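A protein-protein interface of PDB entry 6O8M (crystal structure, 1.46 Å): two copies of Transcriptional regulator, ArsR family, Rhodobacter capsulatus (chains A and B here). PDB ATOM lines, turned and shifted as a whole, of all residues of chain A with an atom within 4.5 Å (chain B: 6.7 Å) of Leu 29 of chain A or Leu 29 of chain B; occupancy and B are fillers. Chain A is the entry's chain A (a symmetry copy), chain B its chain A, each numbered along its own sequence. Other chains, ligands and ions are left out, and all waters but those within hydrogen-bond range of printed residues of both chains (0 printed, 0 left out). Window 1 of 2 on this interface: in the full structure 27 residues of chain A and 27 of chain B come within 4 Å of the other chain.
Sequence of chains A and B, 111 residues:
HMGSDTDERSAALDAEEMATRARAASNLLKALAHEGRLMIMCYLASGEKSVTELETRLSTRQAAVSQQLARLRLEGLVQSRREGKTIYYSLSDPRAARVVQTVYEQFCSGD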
ATOM      1  N   ALA A  25       9.087 -17.642   2.814  1.00  0.00           N
ATOM      2  CA  ALA A  25       8.842 -16.589   1.839  1.00  0.00           C
ATOM      3  C   ALA A  25       9.080 -17.114   0.432  1.00  0.00           C
ATOM      4  O   ALA A  25       8.284 -16.878  -0.481  1.00  0.00           O
ATOM      5  CB  ALA A  25       9.759 -15.395   2.124  1.00  0.00           C
ATOM      6  N   SER A  26      10.198 -17.813   0.233  1.00  0.00           N
ATOM      7  CA  SER A  26      10.510 -18.353  -1.081  1.00  0.00           C
ATOM      8  C   SER A  26       9.427 -19.320  -1.545  1.00  0.00           C
ATOM      9  O   SER A  26       9.085 -19.358  -2.734  1.00  0.00           O
ATOM     10  CB  SER A  26      11.875 -19.033  -1.037  1.00  0.00           C
ATOM     11  OG  SER A  26      12.099 -19.778  -2.208  1.00  0.00           O
ATOM     12  N   ASN A  27       8.870 -20.104  -0.621  1.00  0.00           N
ATOM     13  CA  ASN A  27       7.820 -21.054  -0.986  1.00  0.00           C
ATOM     14  C   ASN A  27       6.524 -20.348  -1.356  1.00  0.00           C
ATOM     15  O   ASN A  27       5.846 -20.749  -2.309  1.00  0.00           O
ATOM     16  CB  ASN A  27       7.582 -22.035   0.157  1.00  0.00           C
ATOM     17  CG  ASN A  27       8.706 -23.032   0.304  1.00  0.00           C
ATOM     18  OD1 ASN A  27       9.503 -23.220  -0.615  1.00  0.00           O
ATOM     19  ND2 ASN A  27       8.786 -23.673   1.468  1.00  0.00           N
ATOM     20  N   LEU A  28       6.144 -19.301  -0.613  1.00  0.00           N
ATOM     21  CA  LEU A  28       4.994 -18.514  -1.037  1.00  0.00           C
ATOM     22  C   LEU A  28       5.216 -17.997  -2.448  1.00  0.00           C
ATOM     23  O   LEU A  28       4.345 -18.105  -3.319  1.00  0.00           O
ATOM     24  CB  LEU A  28       4.741 -17.354  -0.081  1.00  0.00           C
ATOM     25  CG  LEU A  28       3.822 -16.274  -0.653  1.00  0.00           C
ATOM     26  CD1 LEU A  28       2.369 -16.758  -0.837  1.00  0.00           C
ATOM     27  CD2 LEU A  28       3.796 -15.028   0.203  1.00  0.00           C
ATOM     28  N   LEU A  29       6.401 -17.449  -2.708  1.00  0.00           N
ATOM     29  CA  LEU A  29       6.630 -16.859  -4.012  1.00  0.00           C
ATOM     30  C   LEU A  29       6.570 -17.914  -5.111  1.00  0.00           C
ATOM     31  O   LEU A  29       6.047 -17.643  -6.194  1.00  0.00           O
ATOM     32  CB  LEU A  29       7.928 -16.059  -4.004  1.00  0.00           C
ATOM     33  CG  LEU A  29       7.864 -14.848  -3.062  1.00  0.00           C
ATOM     34  CD1 LEU A  29       9.246 -14.265  -2.838  1.00  0.00           C
ATOM     35  CD2 LEU A  29       6.926 -13.801  -3.624  1.00  0.00           C
ATOM     36  N   LYS A  30       7.068 -19.133  -4.848  1.00  0.00           N
ATOM     37  CA  LYS A  30       6.946 -20.202  -5.835  1.00  0.00           C
ATOM     38  C   LYS A  30       5.484 -20.513  -6.130  1.00  0.00           C
ATOM     39  O   LYS A  30       5.113 -20.757  -7.283  1.00  0.00           O
ATOM     40  CB  LYS A  30       7.671 -21.454  -5.354  1.00  0.00           C
ATOM     41  CG  LYS A  30       9.182 -21.305  -5.393  1.00  0.00           C
ATOM     42  CD  LYS A  30       9.907 -22.543  -4.947  1.00  0.00           C
ATOM     43  CE  LYS A  30      11.398 -22.240  -4.852  1.00  0.00           C
ATOM     44  NZ  LYS A  30      12.241 -23.461  -4.866  1.00  0.00           N
ATOM     45  N   ALA A  31       4.641 -20.516  -5.099  1.00  0.00           N
ATOM     46  CA  ALA A  31       3.216 -20.750  -5.316  1.00  0.00           C
ATOM     47  C   ALA A  31       2.586 -19.613  -6.107  1.00  0.00           C
ATOM     48  O   ALA A  31       1.656 -19.837  -6.894  1.00  0.00           O
ATOM     49  CB  ALA A  31       2.497 -20.896  -3.976  1.00  0.00           C
ATOM     50  N   LEU A  32       3.065 -18.384  -5.897  1.00  0.00           N
ATOM     51  CA  LEU A  32       2.510 -17.229  -6.585  1.00  0.00           C
ATOM     52  C   LEU A  32       3.096 -17.045  -7.978  1.00  0.00           C
ATOM     53  O   LEU A  32       2.512 -16.318  -8.783  1.00  0.00           O
ATOM     54  CB  LEU A  32       2.752 -15.953  -5.776  1.00  0.00           C
ATOM     55  CG  LEU A  32       2.142 -15.910  -4.385  1.00  0.00           C
ATOM     56  CD1 LEU A  32       2.490 -14.600  -3.726  1.00  0.00           C
ATOM     57  CD2 LEU A  32       0.620 -16.066  -4.420  1.00  0.00           C
ATOM     58  N   ALA A  33       4.222 -17.689  -8.275  1.00  0.00           N
ATOM     59  CA  ALA A  33       4.971 -17.473  -9.514  1.00  0.00           C
ATOM     60  C   ALA A  33       4.439 -18.320 -10.654  1.00  0.00           C
ATOM     61  O   ALA A  33       5.139 -19.099 -11.296  1.00  0.00           O
ATOM     62  CB  ALA A  33       6.443 -17.757  -9.271  1.00  0.00           C
ATOM     63  N   LEU A  38      -1.560 -16.976  -9.532  1.00  0.00           N
ATOM     64  CA  LEU A  38      -1.503 -15.577  -9.143  1.00  0.00           C
ATOM     65  C   LEU A  38      -2.834 -14.882  -9.381  1.00  0.00           C
ATOM     66  O   LEU A  38      -3.286 -14.097  -8.543  1.00  0.00           O
ATOM     67  CB  LEU A  38      -0.398 -14.872  -9.915  1.00  0.00           C
ATOM     68  CG  LEU A  38      -0.247 -13.391  -9.586  1.00  0.00           C
ATOM     69  CD1 LEU A  38       0.049 -13.192  -8.104  1.00  0.00           C
ATOM     70  CD2 LEU A  38       0.852 -12.769 -10.447  1.00  0.00           C
ATOM     71  N   VAL A 103       1.332  -6.889  -4.883  1.00  0.00           N
ATOM     72  CA  VAL A 103       1.482  -7.249  -6.289  1.00  0.00           C
ATOM     73  C   VAL A 103       0.344  -6.664  -7.113  1.00  0.00           C
ATOM     74  O   VAL A 103       0.560  -6.065  -8.175  1.00  0.00           O
ATOM     75  CB  VAL A 103       1.546  -8.781  -6.439  1.00  0.00           C
ATOM     76  CG1 VAL A 103       1.505  -9.152  -7.895  1.00  0.00           C
ATOM     77  CG2 VAL A 103       2.803  -9.338  -5.782  1.00  0.00           C
ATOM     78  N   ALA B  24       3.956  -9.909 -16.274  1.00  0.00           N
ATOM     79  CA  ALA B  24       5.035  -9.156 -15.647  1.00  0.00           C
ATOM     80  C   ALA B  24       5.094  -9.446 -14.155  1.00  0.00           C
ATOM     81  O   ALA B  24       6.175  -9.651 -13.592  1.00  0.00           O
ATOM     82  CB  ALA B  24       4.842  -7.659 -15.886  1.00  0.00           C
ATOM     83  N   ALA B  25       3.935  -9.486 -13.499  1.00  0.00           N
ATOM     84  CA  ALA B  25       3.908  -9.837 -12.086  1.00  0.00           C
ATOM     85  C   ALA B  25       4.424 -11.253 -11.888  1.00  0.00           C
ATOM     86  O   ALA B  25       5.231 -11.519 -10.993  1.00  0.00           O
ATOM     87  CB  ALA B  25       2.477  -9.712 -11.549  1.00  0.00           C
ATOM     88  N   SER B  26       3.941 -12.188 -12.707  1.00  0.00           N
ATOM     89  CA  SER B  26       4.376 -13.571 -12.589  1.00  0.00           C
ATOM     90  C   SER B  26       5.880 -13.691 -12.801  1.00  0.00           C
ATOM     91  O   SER B  26       6.549 -14.490 -12.135  1.00  0.00           O
ATOM     92  CB  SER B  26       3.609 -14.428 -13.591  1.00  0.00           C
ATOM     93  OG  SER B  26       4.173 -15.713 -13.683  1.00  0.00           O
ATOM     94  N   ASN B  27       6.433 -12.895 -13.719  1.00  0.00           N
ATOM     95  CA  ASN B  27       7.872 -12.946 -13.977  1.00  0.00           C
ATOM     96  C   ASN B  27       8.674 -12.378 -12.813  1.00  0.00           C
ATOM     97  O   ASN B  27       9.721 -12.928 -12.453  1.00  0.00           O
ATOM     98  CB  ASN B  27       8.199 -12.194 -15.262  1.00  0.00           C
ATOM     99  CG  ASN B  27       7.754 -12.943 -16.496  1.00  0.00           C
ATOM    100  OD1 ASN B  27       7.496 -14.145 -16.443  1.00  0.00           O
ATOM    101  ND2 ASN B  27       7.647 -12.232 -17.617  1.00  0.00           N
ATOM    102  N   LEU B  28       8.217 -11.272 -12.216  1.00  0.00           N
ATOM    103  CA  LEU B  28       8.876 -10.798 -11.007  1.00  0.00           C
ATOM    104  C   LEU B  28       8.881 -11.897  -9.958  1.00  0.00           C
ATOM    105  O   LEU B  28       9.910 -12.194  -9.340  1.00  0.00           O
ATOM    106  CB  LEU B  28       8.193  -9.548 -10.463  1.00  0.00           C
ATOM    107  CG  LEU B  28       8.566  -9.224  -9.015  1.00  0.00           C
ATOM    108  CD1 LEU B  28      10.037  -8.783  -8.860  1.00  0.00           C
ATOM    109  CD2 LEU B  28       7.689  -8.144  -8.424  1.00  0.00           C
ATOM    110  N   LEU B  29       7.734 -12.541  -9.759  1.00  0.00           N
ATOM    111  CA  LEU B  29       7.661 -13.535  -8.706  1.00  0.00           C
ATOM    112  C   LEU B  29       8.588 -14.711  -8.996  1.00  0.00           C
ATOM    113  O   LEU B  29       9.212 -15.242  -8.074  1.00  0.00           O
ATOM    114  CB  LEU B  29       6.211 -13.945  -8.470  1.00  0.00           C
ATOM    115  CG  LEU B  29       5.355 -12.787  -7.938  1.00  0.00           C
ATOM    116  CD1 LEU B  29       3.880 -13.129  -8.011  1.00  0.00           C
ATOM    117  CD2 LEU B  29       5.757 -12.454  -6.516  1.00  0.00           C
ATOM    118  N   LYS B  30       8.721 -15.115 -10.269  1.00  0.00           N
ATOM    119  CA  LYS B  30       9.669 -16.173 -10.606  1.00  0.00           C
ATOM    120  C   LYS B  30      11.094 -15.766 -10.253  1.00  0.00           C
ATOM    121  O   LYS B  30      11.879 -16.585  -9.762  1.00  0.00           O
ATOM    122  CB  LYS B  30       9.568 -16.526 -12.086  1.00  0.00           C
ATOM    123  CG  LYS B  30       8.290 -17.275 -12.422  1.00  0.00           C
ATOM    124  CD  LYS B  30       8.192 -17.652 -13.873  1.00  0.00           C
ATOM    125  CE  LYS B  30       6.811 -18.236 -14.144  1.00  0.00           C
ATOM    126  NZ  LYS B  30       6.755 -19.040 -15.390  1.00  0.00           N
ATOM    127  N   ALA B  31      11.449 -14.507 -10.501  1.00  0.00           N
ATOM    128  CA  ALA B  31      12.781 -14.033 -10.134  1.00  0.00           C
ATOM    129  C   ALA B  31      12.962 -14.013  -8.624  1.00  0.00           C
ATOM    130  O   ALA B  31      14.070 -14.249  -8.122  1.00  0.00           O
ATOM    131  CB  ALA B  31      13.011 -12.630 -10.691  1.00  0.00           C
ATOM    132  N   LEU B  32      11.889 -13.718  -7.883  1.00  0.00           N
ATOM    133  CA  LEU B  32      11.969 -13.648  -6.434  1.00  0.00           C
ATOM    134  C   LEU B  32      11.843 -15.016  -5.777  1.00  0.00           C
ATOM    135  O   LEU B  32      12.199 -15.154  -4.606  1.00  0.00           O
ATOM    136  CB  LEU B  32      10.875 -12.733  -5.878  1.00  0.00           C
ATOM    137  CG  LEU B  32      10.906 -11.286  -6.342  1.00  0.00           C
ATOM    138  CD1 LEU B  32       9.758 -10.536  -5.717  1.00  0.00           C
ATOM    139  CD2 LEU B  32      12.220 -10.593  -5.971  1.00  0.00           C
ATOM    140  N   ALA B  33      11.357 -16.018  -6.506  1.00  0.00           N
ATOM    141  CA  ALA B  33      11.035 -17.334  -5.952  1.00  0.00           C
ATOM    142  C   ALA B  33      12.250 -18.242  -5.905  1.00  0.00           C
ATOM    143  O   ALA B  33      12.282 -19.349  -6.436  1.00  0.00           O
ATOM    144  CB  ALA B  33       9.919 -17.966  -6.765  1.00  0.00           C
ATOM    145  N   HIS B  34      13.288 -17.724  -5.283  1.00  0.00           N
ATOM    146  CA  HIS B  34      14.579 -18.387  -5.209  1.00  0.00           C
ATOM    147  C   HIS B  34      15.206 -17.804  -3.959  1.00  0.00           C
ATOM    148  O   HIS B  34      15.279 -16.581  -3.834  1.00  0.00           O
ATOM    149  CB  HIS B  34      15.395 -18.036  -6.437  1.00  0.00           C
ATOM    150  CG  HIS B  34      16.762 -18.617  -6.438  1.00  0.00           C
ATOM    151  ND1 HIS B  34      17.805 -18.075  -5.721  1.00  0.00           N
ATOM    152  CD2 HIS B  34      17.266 -19.685  -7.094  1.00  0.00           C
ATOM    153  CE1 HIS B  34      18.889 -18.799  -5.923  1.00  0.00           C
ATOM    154  NE2 HIS B  34      18.587 -19.781  -6.752  1.00  0.00           N
ATOM    155  N   ARG B  37      18.235 -15.298  -4.503  1.00  0.00           N
ATOM    156  CA  ARG B  37      17.854 -14.031  -5.114  1.00  0.00           C
ATOM    157  C   ARG B  37      16.947 -13.226  -4.198  1.00  0.00           C
ATOM    158  O   ARG B  37      17.057 -11.998  -4.129  1.00  0.00           O
ATOM    159  CB  ARG B  37      17.177 -14.271  -6.460  1.00  0.00           C
ATOM    160  CG  ARG B  37      18.095 -14.892  -7.500  1.00  0.00           C
ATOM    161  CD  ARG B  37      17.566 -14.803  -8.945  1.00  0.00           C
ATOM    162  NE  ARG B  37      16.282 -15.482  -9.135  1.00  0.00           N
ATOM    163  CZ  ARG B  37      16.131 -16.720  -9.585  1.00  0.00           C
ATOM    164  NH1 ARG B  37      17.175 -17.469  -9.909  1.00  0.00           N
ATOM    165  NH2 ARG B  37      14.910 -17.222  -9.708  1.00  0.00           N
ATOM    166  N   LEU B  38      16.039 -13.901  -3.487  1.00  0.00           N
ATOM    167  CA  LEU B  38      15.164 -13.195  -2.565  1.00  0.00           C
ATOM    168  C   LEU B  38      15.958 -12.508  -1.466  1.00  0.00           C
ATOM    169  O   LEU B  38      15.661 -11.367  -1.104  1.00  0.00           O
ATOM    170  CB  LEU B  38      14.163 -14.168  -1.959  1.00  0.00           C
ATOM    171  CG  LEU B  38      13.189 -13.534  -0.971  1.00  0.00           C
ATOM    172  CD1 LEU B  38      12.386 -12.424  -1.639  1.00  0.00           C
ATOM    173  CD2 LEU B  38      12.263 -14.599  -0.387  1.00  0.00           C
ATOM    174  N   VAL B  99       6.957  -4.902  -3.493  1.00  0.00           N
ATOM    175  CA  VAL B  99       6.648  -6.313  -3.261  1.00  0.00           C
ATOM    176  C   VAL B  99       7.638  -6.916  -2.272  1.00  0.00           C
ATOM    177  O   VAL B  99       7.250  -7.580  -1.303  1.00  0.00           O
ATOM    178  CB  VAL B  99       6.624  -7.095  -4.583  1.00  0.00           C
ATOM    179  CG1 VAL B  99       6.524  -8.571  -4.301  1.00  0.00           C
ATOM    180  CG2 VAL B  99       5.432  -6.638  -5.454  1.00  0.00           C
ATOM    181  N   VAL B 103       7.158  -8.575   1.462  1.00  0.00           N
ATOM    182  CA  VAL B 103       7.662  -9.897   1.820  1.00  0.00           C
ATOM    183  C   VAL B 103       8.539  -9.814   3.060  1.00  0.00           C
ATOM    184  O   VAL B 103       8.397 -10.603   4.004  1.00  0.00           O
ATOM    185  CB  VAL B 103       8.430 -10.509   0.635  1.00  0.00           C
ATOM    186  CG1 VAL B 103       9.109 -11.779   1.069  1.00  0.00           C
ATOM    187  CG2 VAL B 103       7.495 -10.779  -0.538  1.00  0.00           C
ATOM    188  N   PHE B 107       7.351 -11.631   6.380  1.00  0.00           N
ATOM    189  CA  PHE B 107       8.024 -12.874   6.721  1.00  0.00           C
ATOM    190  C   PHE B 107       9.080 -12.711   7.795  1.00  0.00           C
ATOM    191  O   PHE B 107       9.463 -13.711   8.412  1.00  0.00           O
ATOM    192  CB  PHE B 107       8.550 -13.558   5.463  1.00  0.00           C
ATOM    193  CG  PHE B 107       7.455 -14.236   4.703  1.00  0.00           C
ATOM    194  CD1 PHE B 107       7.130 -15.544   4.974  1.00  0.00           C
ATOM    195  CD2 PHE B 107       6.689 -13.536   3.790  1.00  0.00           C
ATOM    196  CE1 PHE B 107       6.098 -16.156   4.315  1.00  0.00           C
ATOM    197  CE2 PHE B 107       5.635 -14.148   3.138  1.00  0.00           C
ATOM    198  CZ  PHE B 107       5.351 -15.458   3.393  1.00  0.00           C
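Ala 25 of chain A touches Val 103 of chain B, and with the chains exchanged Val 103 of chain A touches Ala 25 of chain B. Leu 29 of chain A touches its own counterpart, Leu 29 of chain B. Leu 29 of chain A touches Leu 32 of chain B, and with the chains exchanged Leu 32 of chain A touches Leu 29 of chain B. Leu 29 of chain A touches Leu 38 of chain B, and with the chains exchanged Leu 38 of chain A touches Leu 29 of chain B.
Of the 11 printed residues of chain A, 9 touch a printed residue of chain B. Printed residues of chain A that touch a printed residue of chain B: Ala 25, Ser 26, Leu 28, Leu 29, Lys 30, Leu 32, Ala 33, Leu 38 and Val 103. Hydrophobic or aromatic side chains of chain A within 4 Å of the printed part of chain B: Ala 25, Leu 28, Leu 29, Leu 32, Ala 33, Leu 38 and Val 103. Of the 16 printed residues of chain B, 11 touch a printed residue of chain A. Hydrophobic or aromatic side chains of chain B that line the printed part of chain A: Ala 25, Leu 29, Leu 32, Ala 33, Leu 38, Val 99, Val 103 and Phe 107. Among the printed residues, 19 pairs touch across the chains.
A ring nitrogen (ND1) of His 34 of chain B sits at hydrogen-bond distance from the backbone NH of Arg 37 of chain B (3.1 Å). The guanidinium group (NH2) of Arg 37 of chain B sits at hydrogen-bond distance from the backbone carbonyl oxygen (O) of Lys 30 of chain B, 3.1 Å away.
Among the printed residues, pairs that only touch across the chains: Leu 29 of chain A with Leu 29 of chain B, Lys 30 of chain A with Ala 33 of chain B, Ala 33 of chain A with Lys 30 of chain B, Leu 29 of chain A with Leu 32 of chain B, Leu 32 of chain A with Leu 29 of chain B, Leu 28 of chain A with Phe 107 of chain B, Ala 25 of chain A with Phe 107 of chain B, Leu 38 of chain A with Ala 25 of chain B, Ala 25 of chain A with Leu 38 of chain B, Leu 29 of chain A with Ala 33 of chain B, Ala 33 of chain A with Leu 29 of chain B, Val 103 of chain A with Val 99 of chain B, Val 103 of chain A with Ala 25 of chain B, Ala 25 of chain A with Val 103 of chain B, Leu 29 of chain A with Leu 38 of chain B, Leu 38 of chain A with Leu 29 of chain B, Ser 26 of chain A with Leu 38 of chain B, Leu 38 of chain A with Ser 26 of chain B and Ser 26 of chain A with His 34 of chain B.
Leu 29 of chain A touches four residues of chain B. Of the printed residues of chain B, Val 103 of chain A touches Ala 25 and Val 99. Of chain A, only Leu 29, Leu 32, Ala 33 and Leu 38 come within 4 Å of Leu 29 of chain B. Of the printed residues of chain A, Ala 33 of chain B touches Leu 29 and Lys 30. Of the printed residues of chain A, His 34 of chain B touches Ser 26. Printed residues of chain A within 4 Å of Leu 38 of chain B: Ala 25 (3.6 Å), Ser 26 (3.9 Å) and Leu 29 (3.8 Å). Of the printed residues of chain A, Val 99 of chain B touches Val 103 (3.8 Å). The nearest residue of chain B that does not touch Leu 29 of chain A is Val 103 of chain B (4.4 Å). The nearest residue of chain A that does not touch Leu 29 of chain B is Val 103 of chain A (4.4 Å).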
